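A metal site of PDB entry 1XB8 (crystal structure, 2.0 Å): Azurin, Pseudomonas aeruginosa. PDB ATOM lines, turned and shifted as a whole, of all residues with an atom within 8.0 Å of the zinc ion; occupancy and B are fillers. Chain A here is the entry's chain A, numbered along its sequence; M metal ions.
The backbone NH of Ile 87 is in hydrogen-bond range of the backbone carbonyl oxygen of His 46. A ring nitrogen (NE2) of His 117 lies close to the side-chain sulfur (SD) of Met 44. The side-chain sulfur (SG) of Cys 112 lies close to the side-chain amide oxygen (OD1) of Asn 47 (3.4 Å). A ring nitrogen (ND1) of His 46 sits close to the side-chain sulfur of Met 121 (3.3 Å). The side-chain sulfur (SG) of Cys 112 sits close to the backbone NH (N) of Phe 114, at 3.4 Å. NE2 of His 46 sits at hydrogen-bond distance from O of Asn 10, 2.7 Å away. N of Cys 112 lies within hydrogen-bond range of O of Met 121. O of Cys 112 sits close to N of Ser 118, at 3.4 Å.
The zinc ion is bound by ND1 of His 117 (2.1 Å), ND1 of His 46 (2.1 Å), O of Gly 45 (2.2 Å) and SG of Cys 112 (2.3 Å).
CB of Phe 114 touches the zinc ion, at 3.6 Å. Met 121 touches the zinc ion. Along chain A the residues within 4 Å of the zinc ion span positions 45 to 121.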
ATOM      1  N   GLY A   9      14.571 -28.368  -0.728  1.00  0.00           N
ATOM      2  CA  GLY A   9      15.462 -27.382  -0.145  1.00  0.00           C
ATOM      3  C   GLY A   9      16.493 -28.183   0.619  1.00  0.00           C
ATOM      4  O   GLY A   9      16.133 -28.986   1.435  1.00  0.00           O
ATOM      5  N   ASN A  10      17.765 -27.950   0.328  1.00  0.00           N
ATOM      6  CA  ASN A  10      18.839 -28.884   0.778  1.00  0.00           C
ATOM      7  C   ASN A  10      19.609 -28.300   1.983  1.00  0.00           C
ATOM      8  O   ASN A  10      19.197 -27.285   2.544  1.00  0.00           O
ATOM      9  CB  ASN A  10      19.749 -29.293  -0.428  1.00  0.00           C
ATOM     10  CG  ASN A  10      20.639 -28.155  -0.935  1.00  0.00           C
ATOM     11  OD1 ASN A  10      20.818 -27.150  -0.270  1.00  0.00           O
ATOM     12  ND2 ASN A  10      21.238 -28.345  -2.106  1.00  0.00           N
ATOM     13  N   MET A  13      21.444 -24.451   1.793  1.00  0.00           N
ATOM     14  CA  MET A  13      20.552 -23.300   1.558  1.00  0.00           C
ATOM     15  C   MET A  13      20.210 -23.054   0.109  1.00  0.00           C
ATOM     16  O   MET A  13      20.398 -21.963  -0.405  1.00  0.00           O
ATOM     17  CB  MET A  13      21.154 -22.035   2.110  1.00  0.00           C
ATOM     18  CG  MET A  13      21.350 -22.097   3.574  1.00  0.00           C
ATOM     19  SD  MET A  13      23.081 -22.226   3.978  1.00  0.00           S
ATOM     20  CE  MET A  13      23.090 -20.630   4.827  1.00  0.00           C
ATOM     21  N   GLN A  14      19.699 -24.083  -0.543  1.00  0.00           N
ATOM     22  CA  GLN A  14      19.409 -23.994  -1.938  1.00  0.00           C
ATOM     23  C   GLN A  14      18.049 -24.641  -2.224  1.00  0.00           C
ATOM     24  O   GLN A  14      17.784 -25.731  -1.723  1.00  0.00           O
ATOM     25  CB  GLN A  14      20.562 -24.726  -2.653  1.00  0.00           C
ATOM     26  CG  GLN A  14      20.953 -24.227  -3.957  1.00  0.00           C
ATOM     27  CD  GLN A  14      21.761 -22.958  -3.990  1.00  0.00           C
ATOM     28  OE1 GLN A  14      21.580 -22.012  -3.177  1.00  0.00           O
ATOM     29  NE2 GLN A  14      22.593 -22.870  -5.019  1.00  0.00           N
ATOM     30  N   PHE A  15      17.225 -23.965  -3.035  1.00  0.00           N
ATOM     31  CA  PHE A  15      16.078 -24.600  -3.675  1.00  0.00           C
ATOM     32  C   PHE A  15      16.526 -25.236  -5.025  1.00  0.00           C
ATOM     33  O   PHE A  15      17.444 -24.720  -5.651  1.00  0.00           O
ATOM     34  CB  PHE A  15      14.978 -23.575  -3.952  1.00  0.00           C
ATOM     35  CG  PHE A  15      14.098 -23.207  -2.753  1.00  0.00           C
ATOM     36  CD1 PHE A  15      13.773 -21.897  -2.520  1.00  0.00           C
ATOM     37  CD2 PHE A  15      13.493 -24.178  -1.957  1.00  0.00           C
ATOM     38  CE1 PHE A  15      12.924 -21.537  -1.454  1.00  0.00           C
ATOM     39  CE2 PHE A  15      12.657 -23.849  -0.906  1.00  0.00           C
ATOM     40  CZ  PHE A  15      12.350 -22.533  -0.659  1.00  0.00           C
ATOM     41  N   LEU A  33       6.865 -29.543  -1.075  1.00  0.00           N
ATOM     42  CA  LEU A  33       8.218 -29.266  -0.566  1.00  0.00           C
ATOM     43  C   LEU A  33       8.792 -30.400   0.276  1.00  0.00           C
ATOM     44  O   LEU A  33       8.110 -30.979   1.119  1.00  0.00           O
ATOM     45  CB  LEU A  33       8.237 -27.971   0.281  1.00  0.00           C
ATOM     46  CG  LEU A  33       9.616 -27.508   0.817  1.00  0.00           C
ATOM     47  CD1 LEU A  33      10.521 -26.924  -0.263  1.00  0.00           C
ATOM     48  CD2 LEU A  33       9.376 -26.480   1.930  1.00  0.00           C
ATOM     49  N   HIS A  35      12.883 -31.880   1.979  1.00  0.00           N
ATOM     50  CA  HIS A  35      14.157 -31.419   2.531  1.00  0.00           C
ATOM     51  C   HIS A  35      15.127 -32.599   2.584  1.00  0.00           C
ATOM     52  O   HIS A  35      15.279 -33.257   3.630  1.00  0.00           O
ATOM     53  CB  HIS A  35      13.952 -30.884   3.945  1.00  0.00           C
ATOM     54  CG  HIS A  35      15.139 -30.136   4.512  1.00  0.00           C
ATOM     55  ND1 HIS A  35      16.455 -30.554   4.383  1.00  0.00           N
ATOM     56  CD2 HIS A  35      15.182 -29.029   5.298  1.00  0.00           C
ATOM     57  CE1 HIS A  35      17.248 -29.718   5.031  1.00  0.00           C
ATOM     58  NE2 HIS A  35      16.494 -28.785   5.613  1.00  0.00           N
ATOM     59  N   LYS A  41      15.111 -28.622  11.563  1.00  0.00           N
ATOM     60  CA  LYS A  41      14.452 -27.391  11.120  1.00  0.00           C
ATOM     61  C   LYS A  41      14.917 -26.153  11.895  1.00  0.00           C
ATOM     62  O   LYS A  41      14.938 -25.074  11.329  1.00  0.00           O
ATOM     63  CB  LYS A  41      12.915 -27.504  11.122  1.00  0.00           C
ATOM     64  CG  LYS A  41      12.275 -27.725  12.461  1.00  0.00           C
ATOM     65  CD  LYS A  41      10.788 -27.696  12.325  1.00  0.00           C
ATOM     66  CE  LYS A  41      10.083 -27.636  13.676  1.00  0.00           C
ATOM     67  NZ  LYS A  41       8.650 -28.106  13.518  1.00  0.00           N
ATOM     68  N   VAL A  43      17.941 -25.373  12.665  1.00  0.00           N
ATOM     69  CA  VAL A  43      19.250 -24.998  12.101  1.00  0.00           C
ATOM     70  C   VAL A  43      19.273 -24.734  10.569  1.00  0.00           C
ATOM     71  O   VAL A  43      20.104 -23.949  10.091  1.00  0.00           O
ATOM     72  CB  VAL A  43      20.295 -26.091  12.517  1.00  0.00           C
ATOM     73  CG1 VAL A  43      21.483 -26.170  11.609  1.00  0.00           C
ATOM     74  CG2 VAL A  43      20.786 -25.814  13.899  1.00  0.00           C
ATOM     75  N   MET A  44      18.342 -25.360   9.831  1.00  0.00           N
ATOM     76  CA  MET A  44      18.289 -25.330   8.373  1.00  0.00           C
ATOM     77  C   MET A  44      16.835 -25.540   7.944  1.00  0.00           C
ATOM     78  O   MET A  44      16.522 -26.329   7.069  1.00  0.00           O
ATOM     79  CB  MET A  44      19.163 -26.478   7.811  1.00  0.00           C
ATOM     80  CG  MET A  44      19.425 -26.474   6.295  1.00  0.00           C
ATOM     81  SD  MET A  44      20.252 -24.988   5.684  1.00  0.00           S
ATOM     82  CE  MET A  44      21.829 -24.994   6.506  1.00  0.00           C
ATOM     83  N   GLY A  45      15.927 -24.825   8.583  1.00  0.00           N
ATOM     84  CA  GLY A  45      14.514 -25.003   8.263  1.00  0.00           C
ATOM     85  C   GLY A  45      14.264 -24.396   6.915  1.00  0.00           C
ATOM     86  O   GLY A  45      14.936 -23.429   6.542  1.00  0.00           O
ATOM     87  N   HIS A  46      13.326 -25.000   6.183  1.00  0.00           N
ATOM     88  CA  HIS A  46      12.861 -24.420   4.927  1.00  0.00           C
ATOM     89  C   HIS A  46      11.349 -24.423   4.912  1.00  0.00           C
ATOM     90  O   HIS A  46      10.729 -25.377   5.344  1.00  0.00           O
ATOM     91  CB  HIS A  46      13.394 -25.188   3.679  1.00  0.00           C
ATOM     92  CG  HIS A  46      14.907 -25.323   3.614  1.00  0.00           C
ATOM     93  ND1 HIS A  46      15.780 -24.277   3.832  1.00  0.00           N
ATOM     94  CD2 HIS A  46      15.681 -26.374   3.252  1.00  0.00           C
ATOM     95  CE1 HIS A  46      17.021 -24.675   3.641  1.00  0.00           C
ATOM     96  NE2 HIS A  46      17.001 -25.946   3.300  1.00  0.00           N
ATOM     97  N   ASN A  47      10.802 -23.293   4.449  1.00  0.00           N
ATOM     98  CA  ASN A  47       9.431 -23.153   4.029  1.00  0.00           C
ATOM     99  C   ASN A  47       9.450 -22.584   2.604  1.00  0.00           C
ATOM    100  O   ASN A  47      10.512 -22.192   2.053  1.00  0.00           O
ATOM    101  CB  ASN A  47       8.586 -22.241   4.982  1.00  0.00           C
ATOM    102  CG  ASN A  47       9.240 -20.895   5.274  1.00  0.00           C
ATOM    103  OD1 ASN A  47      10.203 -20.528   4.615  1.00  0.00           O
ATOM    104  ND2 ASN A  47       8.690 -20.128   6.260  1.00  0.00           N
ATOM    105  N   TRP A  48       8.291 -22.608   1.976  1.00  0.00           N
ATOM    106  CA  TRP A  48       8.116 -22.054   0.646  1.00  0.00           C
ATOM    107  C   TRP A  48       6.981 -21.076   0.871  1.00  0.00           C
ATOM    108  O   TRP A  48       5.883 -21.446   1.318  1.00  0.00           O
ATOM    109  CB  TRP A  48       7.754 -23.150  -0.376  1.00  0.00           C
ATOM    110  CG  TRP A  48       7.554 -22.641  -1.752  1.00  0.00           C
ATOM    111  CD1 TRP A  48       8.474 -22.619  -2.709  1.00  0.00           C
ATOM    112  CD2 TRP A  48       6.344 -22.102  -2.334  1.00  0.00           C
ATOM    113  NE1 TRP A  48       7.948 -22.112  -3.876  1.00  0.00           N
ATOM    114  CE2 TRP A  48       6.636 -21.768  -3.664  1.00  0.00           C
ATOM    115  CE3 TRP A  48       5.057 -21.857  -1.854  1.00  0.00           C
ATOM    116  CZ2 TRP A  48       5.663 -21.239  -4.547  1.00  0.00           C
ATOM    117  CZ3 TRP A  48       4.094 -21.269  -2.714  1.00  0.00           C
ATOM    118  CH2 TRP A  48       4.416 -20.977  -4.049  1.00  0.00           C
ATOM    119  N   TYR A  72       8.809 -18.683  11.448  1.00  0.00           N
ATOM    120  CA  TYR A  72       9.389 -17.463  10.865  1.00  0.00           C
ATOM    121  C   TYR A  72       8.456 -16.775   9.864  1.00  0.00           C
ATOM    122  O   TYR A  72       8.878 -16.257   8.824  1.00  0.00           O
ATOM    123  CB  TYR A  72      10.774 -17.762  10.270  1.00  0.00           C
ATOM    124  CG  TYR A  72      11.813 -18.213  11.286  1.00  0.00           C
ATOM    125  CD1 TYR A  72      12.352 -17.310  12.212  1.00  0.00           C
ATOM    126  CD2 TYR A  72      12.295 -19.511  11.289  1.00  0.00           C
ATOM    127  CE1 TYR A  72      13.330 -17.709  13.143  1.00  0.00           C
ATOM    128  CE2 TYR A  72      13.270 -19.913  12.211  1.00  0.00           C
ATOM    129  CZ  TYR A  72      13.783 -19.009  13.122  1.00  0.00           C
ATOM    130  OH  TYR A  72      14.747 -19.408  14.002  1.00  0.00           O
ATOM    131  N   LEU A  86       7.251 -24.676   7.970  1.00  0.00           N
ATOM    132  CA  LEU A  86       8.710 -24.815   8.059  1.00  0.00           C
ATOM    133  C   LEU A  86       9.125 -26.289   8.299  1.00  0.00           C
ATOM    134  O   LEU A  86       8.701 -26.934   9.246  1.00  0.00           O
ATOM    135  CB  LEU A  86       9.194 -23.934   9.218  1.00  0.00           C
ATOM    136  CG  LEU A  86      10.710 -23.801   9.280  1.00  0.00           C
ATOM    137  CD1 LEU A  86      11.223 -22.767   8.286  1.00  0.00           C
ATOM    138  CD2 LEU A  86      11.132 -23.513  10.707  1.00  0.00           C
ATOM    139  N   ILE A  87       9.992 -26.832   7.429  1.00  0.00           N
ATOM    140  CA  ILE A  87      10.376 -28.248   7.565  1.00  0.00           C
ATOM    141  C   ILE A  87      11.889 -28.417   7.713  1.00  0.00           C
ATOM    142  O   ILE A  87      12.658 -27.536   7.329  1.00  0.00           O
ATOM    143  CB  ILE A  87       9.813 -29.115   6.388  1.00  0.00           C
ATOM    144  CG1 ILE A  87      10.347 -28.662   5.031  1.00  0.00           C
ATOM    145  CG2 ILE A  87       8.305 -29.082   6.395  1.00  0.00           C
ATOM    146  CD1 ILE A  87      10.251 -29.733   3.916  1.00  0.00           C
ATOM    147  N   PHE A 111      10.180 -17.860  -1.641  1.00  0.00           N
ATOM    148  CA  PHE A 111      11.352 -17.835  -0.845  1.00  0.00           C
ATOM    149  C   PHE A 111      11.154 -18.588   0.494  1.00  0.00           C
ATOM    150  O   PHE A 111      10.025 -18.918   0.916  1.00  0.00           O
ATOM    151  CB  PHE A 111      11.727 -16.356  -0.554  1.00  0.00           C
ATOM    152  CG  PHE A 111      10.559 -15.529  -0.129  1.00  0.00           C
ATOM    153  CD1 PHE A 111       9.704 -14.951  -1.054  1.00  0.00           C
ATOM    154  CD2 PHE A 111      10.311 -15.310   1.215  1.00  0.00           C
ATOM    155  CE1 PHE A 111       8.600 -14.156  -0.668  1.00  0.00           C
ATOM    156  CE2 PHE A 111       9.253 -14.507   1.609  1.00  0.00           C
ATOM    157  CZ  PHE A 111       8.394 -13.934   0.665  1.00  0.00           C
ATOM    158  N   CYS A 112      12.305 -18.807   1.150  1.00  0.00           N
ATOM    159  CA  CYS A 112      12.349 -19.332   2.515  1.00  0.00           C
ATOM    160  C   CYS A 112      12.618 -18.160   3.421  1.00  0.00           C
ATOM    161  O   CYS A 112      13.436 -17.297   3.052  1.00  0.00           O
ATOM    162  CB  CYS A 112      13.468 -20.350   2.668  1.00  0.00           C
ATOM    163  SG  CYS A 112      13.549 -20.990   4.345  1.00  0.00           S
ATOM    164  N   THR A 113      11.854 -18.074   4.522  1.00  0.00           N
ATOM    165  CA  THR A 113      11.957 -16.991   5.504  1.00  0.00           C
ATOM    166  C   THR A 113      12.727 -17.409   6.758  1.00  0.00           C
ATOM    167  O   THR A 113      12.830 -16.623   7.696  1.00  0.00           O
ATOM    168  CB  THR A 113      10.604 -16.465   5.995  1.00  0.00           C
ATOM    169  OG1 THR A 113       9.897 -17.510   6.634  1.00  0.00           O
ATOM    170  CG2 THR A 113       9.744 -15.906   4.820  1.00  0.00           C
ATOM    171  N   PHE A 114      13.314 -18.596   6.768  1.00  0.00           N
ATOM    172  CA  PHE A 114      14.269 -18.976   7.816  1.00  0.00           C
ATOM    173  C   PHE A 114      15.433 -17.999   7.844  1.00  0.00           C
ATOM    174  O   PHE A 114      15.951 -17.615   6.776  1.00  0.00           O
ATOM    175  CB  PHE A 114      14.782 -20.390   7.632  1.00  0.00           C
ATOM    176  CG  PHE A 114      15.641 -20.871   8.764  1.00  0.00           C
ATOM    177  CD1 PHE A 114      15.118 -21.605   9.814  1.00  0.00           C
ATOM    178  CD2 PHE A 114      16.983 -20.587   8.783  1.00  0.00           C
ATOM    179  CE1 PHE A 114      15.945 -22.046  10.890  1.00  0.00           C
ATOM    180  CE2 PHE A 114      17.774 -21.024   9.834  1.00  0.00           C
ATOM    181  CZ  PHE A 114      17.239 -21.757  10.865  1.00  0.00           C
ATOM    182  N   PRO A 115      15.850 -17.574   9.063  1.00  0.00           N
ATOM    183  CA  PRO A 115      16.865 -16.526   9.127  1.00  0.00           C
ATOM    184  C   PRO A 115      18.015 -16.776   8.202  1.00  0.00           C
ATOM    185  O   PRO A 115      18.670 -17.819   8.283  1.00  0.00           O
ATOM    186  CB  PRO A 115      17.371 -16.607  10.596  1.00  0.00           C
ATOM    187  CG  PRO A 115      16.212 -17.196  11.376  1.00  0.00           C
ATOM    188  CD  PRO A 115      15.415 -18.018  10.404  1.00  0.00           C
ATOM    189  N   GLY A 116      18.248 -15.830   7.322  1.00  0.00           N
ATOM    190  CA  GLY A 116      19.381 -15.866   6.437  1.00  0.00           C
ATOM    191  C   GLY A 116      19.217 -16.689   5.172  1.00  0.00           C
ATOM    192  O   GLY A 116      20.159 -16.800   4.408  1.00  0.00           O
ATOM    193  N   HIS A 117      18.063 -17.308   4.956  1.00  0.00           N
ATOM    194  CA  HIS A 117      17.945 -18.187   3.771  1.00  0.00           C
ATOM    195  C   HIS A 117      17.396 -17.458   2.536  1.00  0.00           C
ATOM    196  O   HIS A 117      17.635 -17.892   1.447  1.00  0.00           O
ATOM    197  CB  HIS A 117      17.068 -19.401   4.083  1.00  0.00           C
ATOM    198  CG  HIS A 117      17.750 -20.405   4.979  1.00  0.00           C
ATOM    199  ND1 HIS A 117      17.164 -21.614   5.314  1.00  0.00           N
ATOM    200  CD2 HIS A 117      18.955 -20.387   5.587  1.00  0.00           C
ATOM    201  CE1 HIS A 117      17.964 -22.271   6.126  1.00  0.00           C
ATOM    202  NE2 HIS A 117      19.067 -21.558   6.306  1.00  0.00           N
ATOM    203  N   SER A 118      16.683 -16.346   2.727  1.00  0.00           N
ATOM    204  CA  SER A 118      15.934 -15.717   1.601  1.00  0.00           C
ATOM    205  C   SER A 118      16.763 -15.193   0.439  1.00  0.00           C
ATOM    206  O   SER A 118      16.249 -15.110  -0.697  1.00  0.00           O
ATOM    207  CB  SER A 118      15.033 -14.586   2.110  1.00  0.00           C
ATOM    208  OG  SER A 118      15.814 -13.512   2.630  1.00  0.00           O
ATOM    209  N   MET A 121      17.682 -18.509  -1.261  1.00  0.00           N
ATOM    210  CA  MET A 121      16.545 -19.420  -1.452  1.00  0.00           C
ATOM    211  C   MET A 121      15.358 -18.623  -1.836  1.00  0.00           C
ATOM    212  O   MET A 121      14.487 -18.334  -1.011  1.00  0.00           O
ATOM    213  CB  MET A 121      16.268 -20.191  -0.142  1.00  0.00           C
ATOM    214  CG  MET A 121      17.391 -21.175   0.203  1.00  0.00           C
ATOM    215  SD  MET A 121      16.935 -22.269   1.541  1.00  0.00           S
ATOM    216  CE  MET A 121      15.936 -23.538   0.703  1.00  0.00           C
HETATM  217 ZN    ZN M   1      15.360 -22.367   4.654  1.00  0.00          ZN
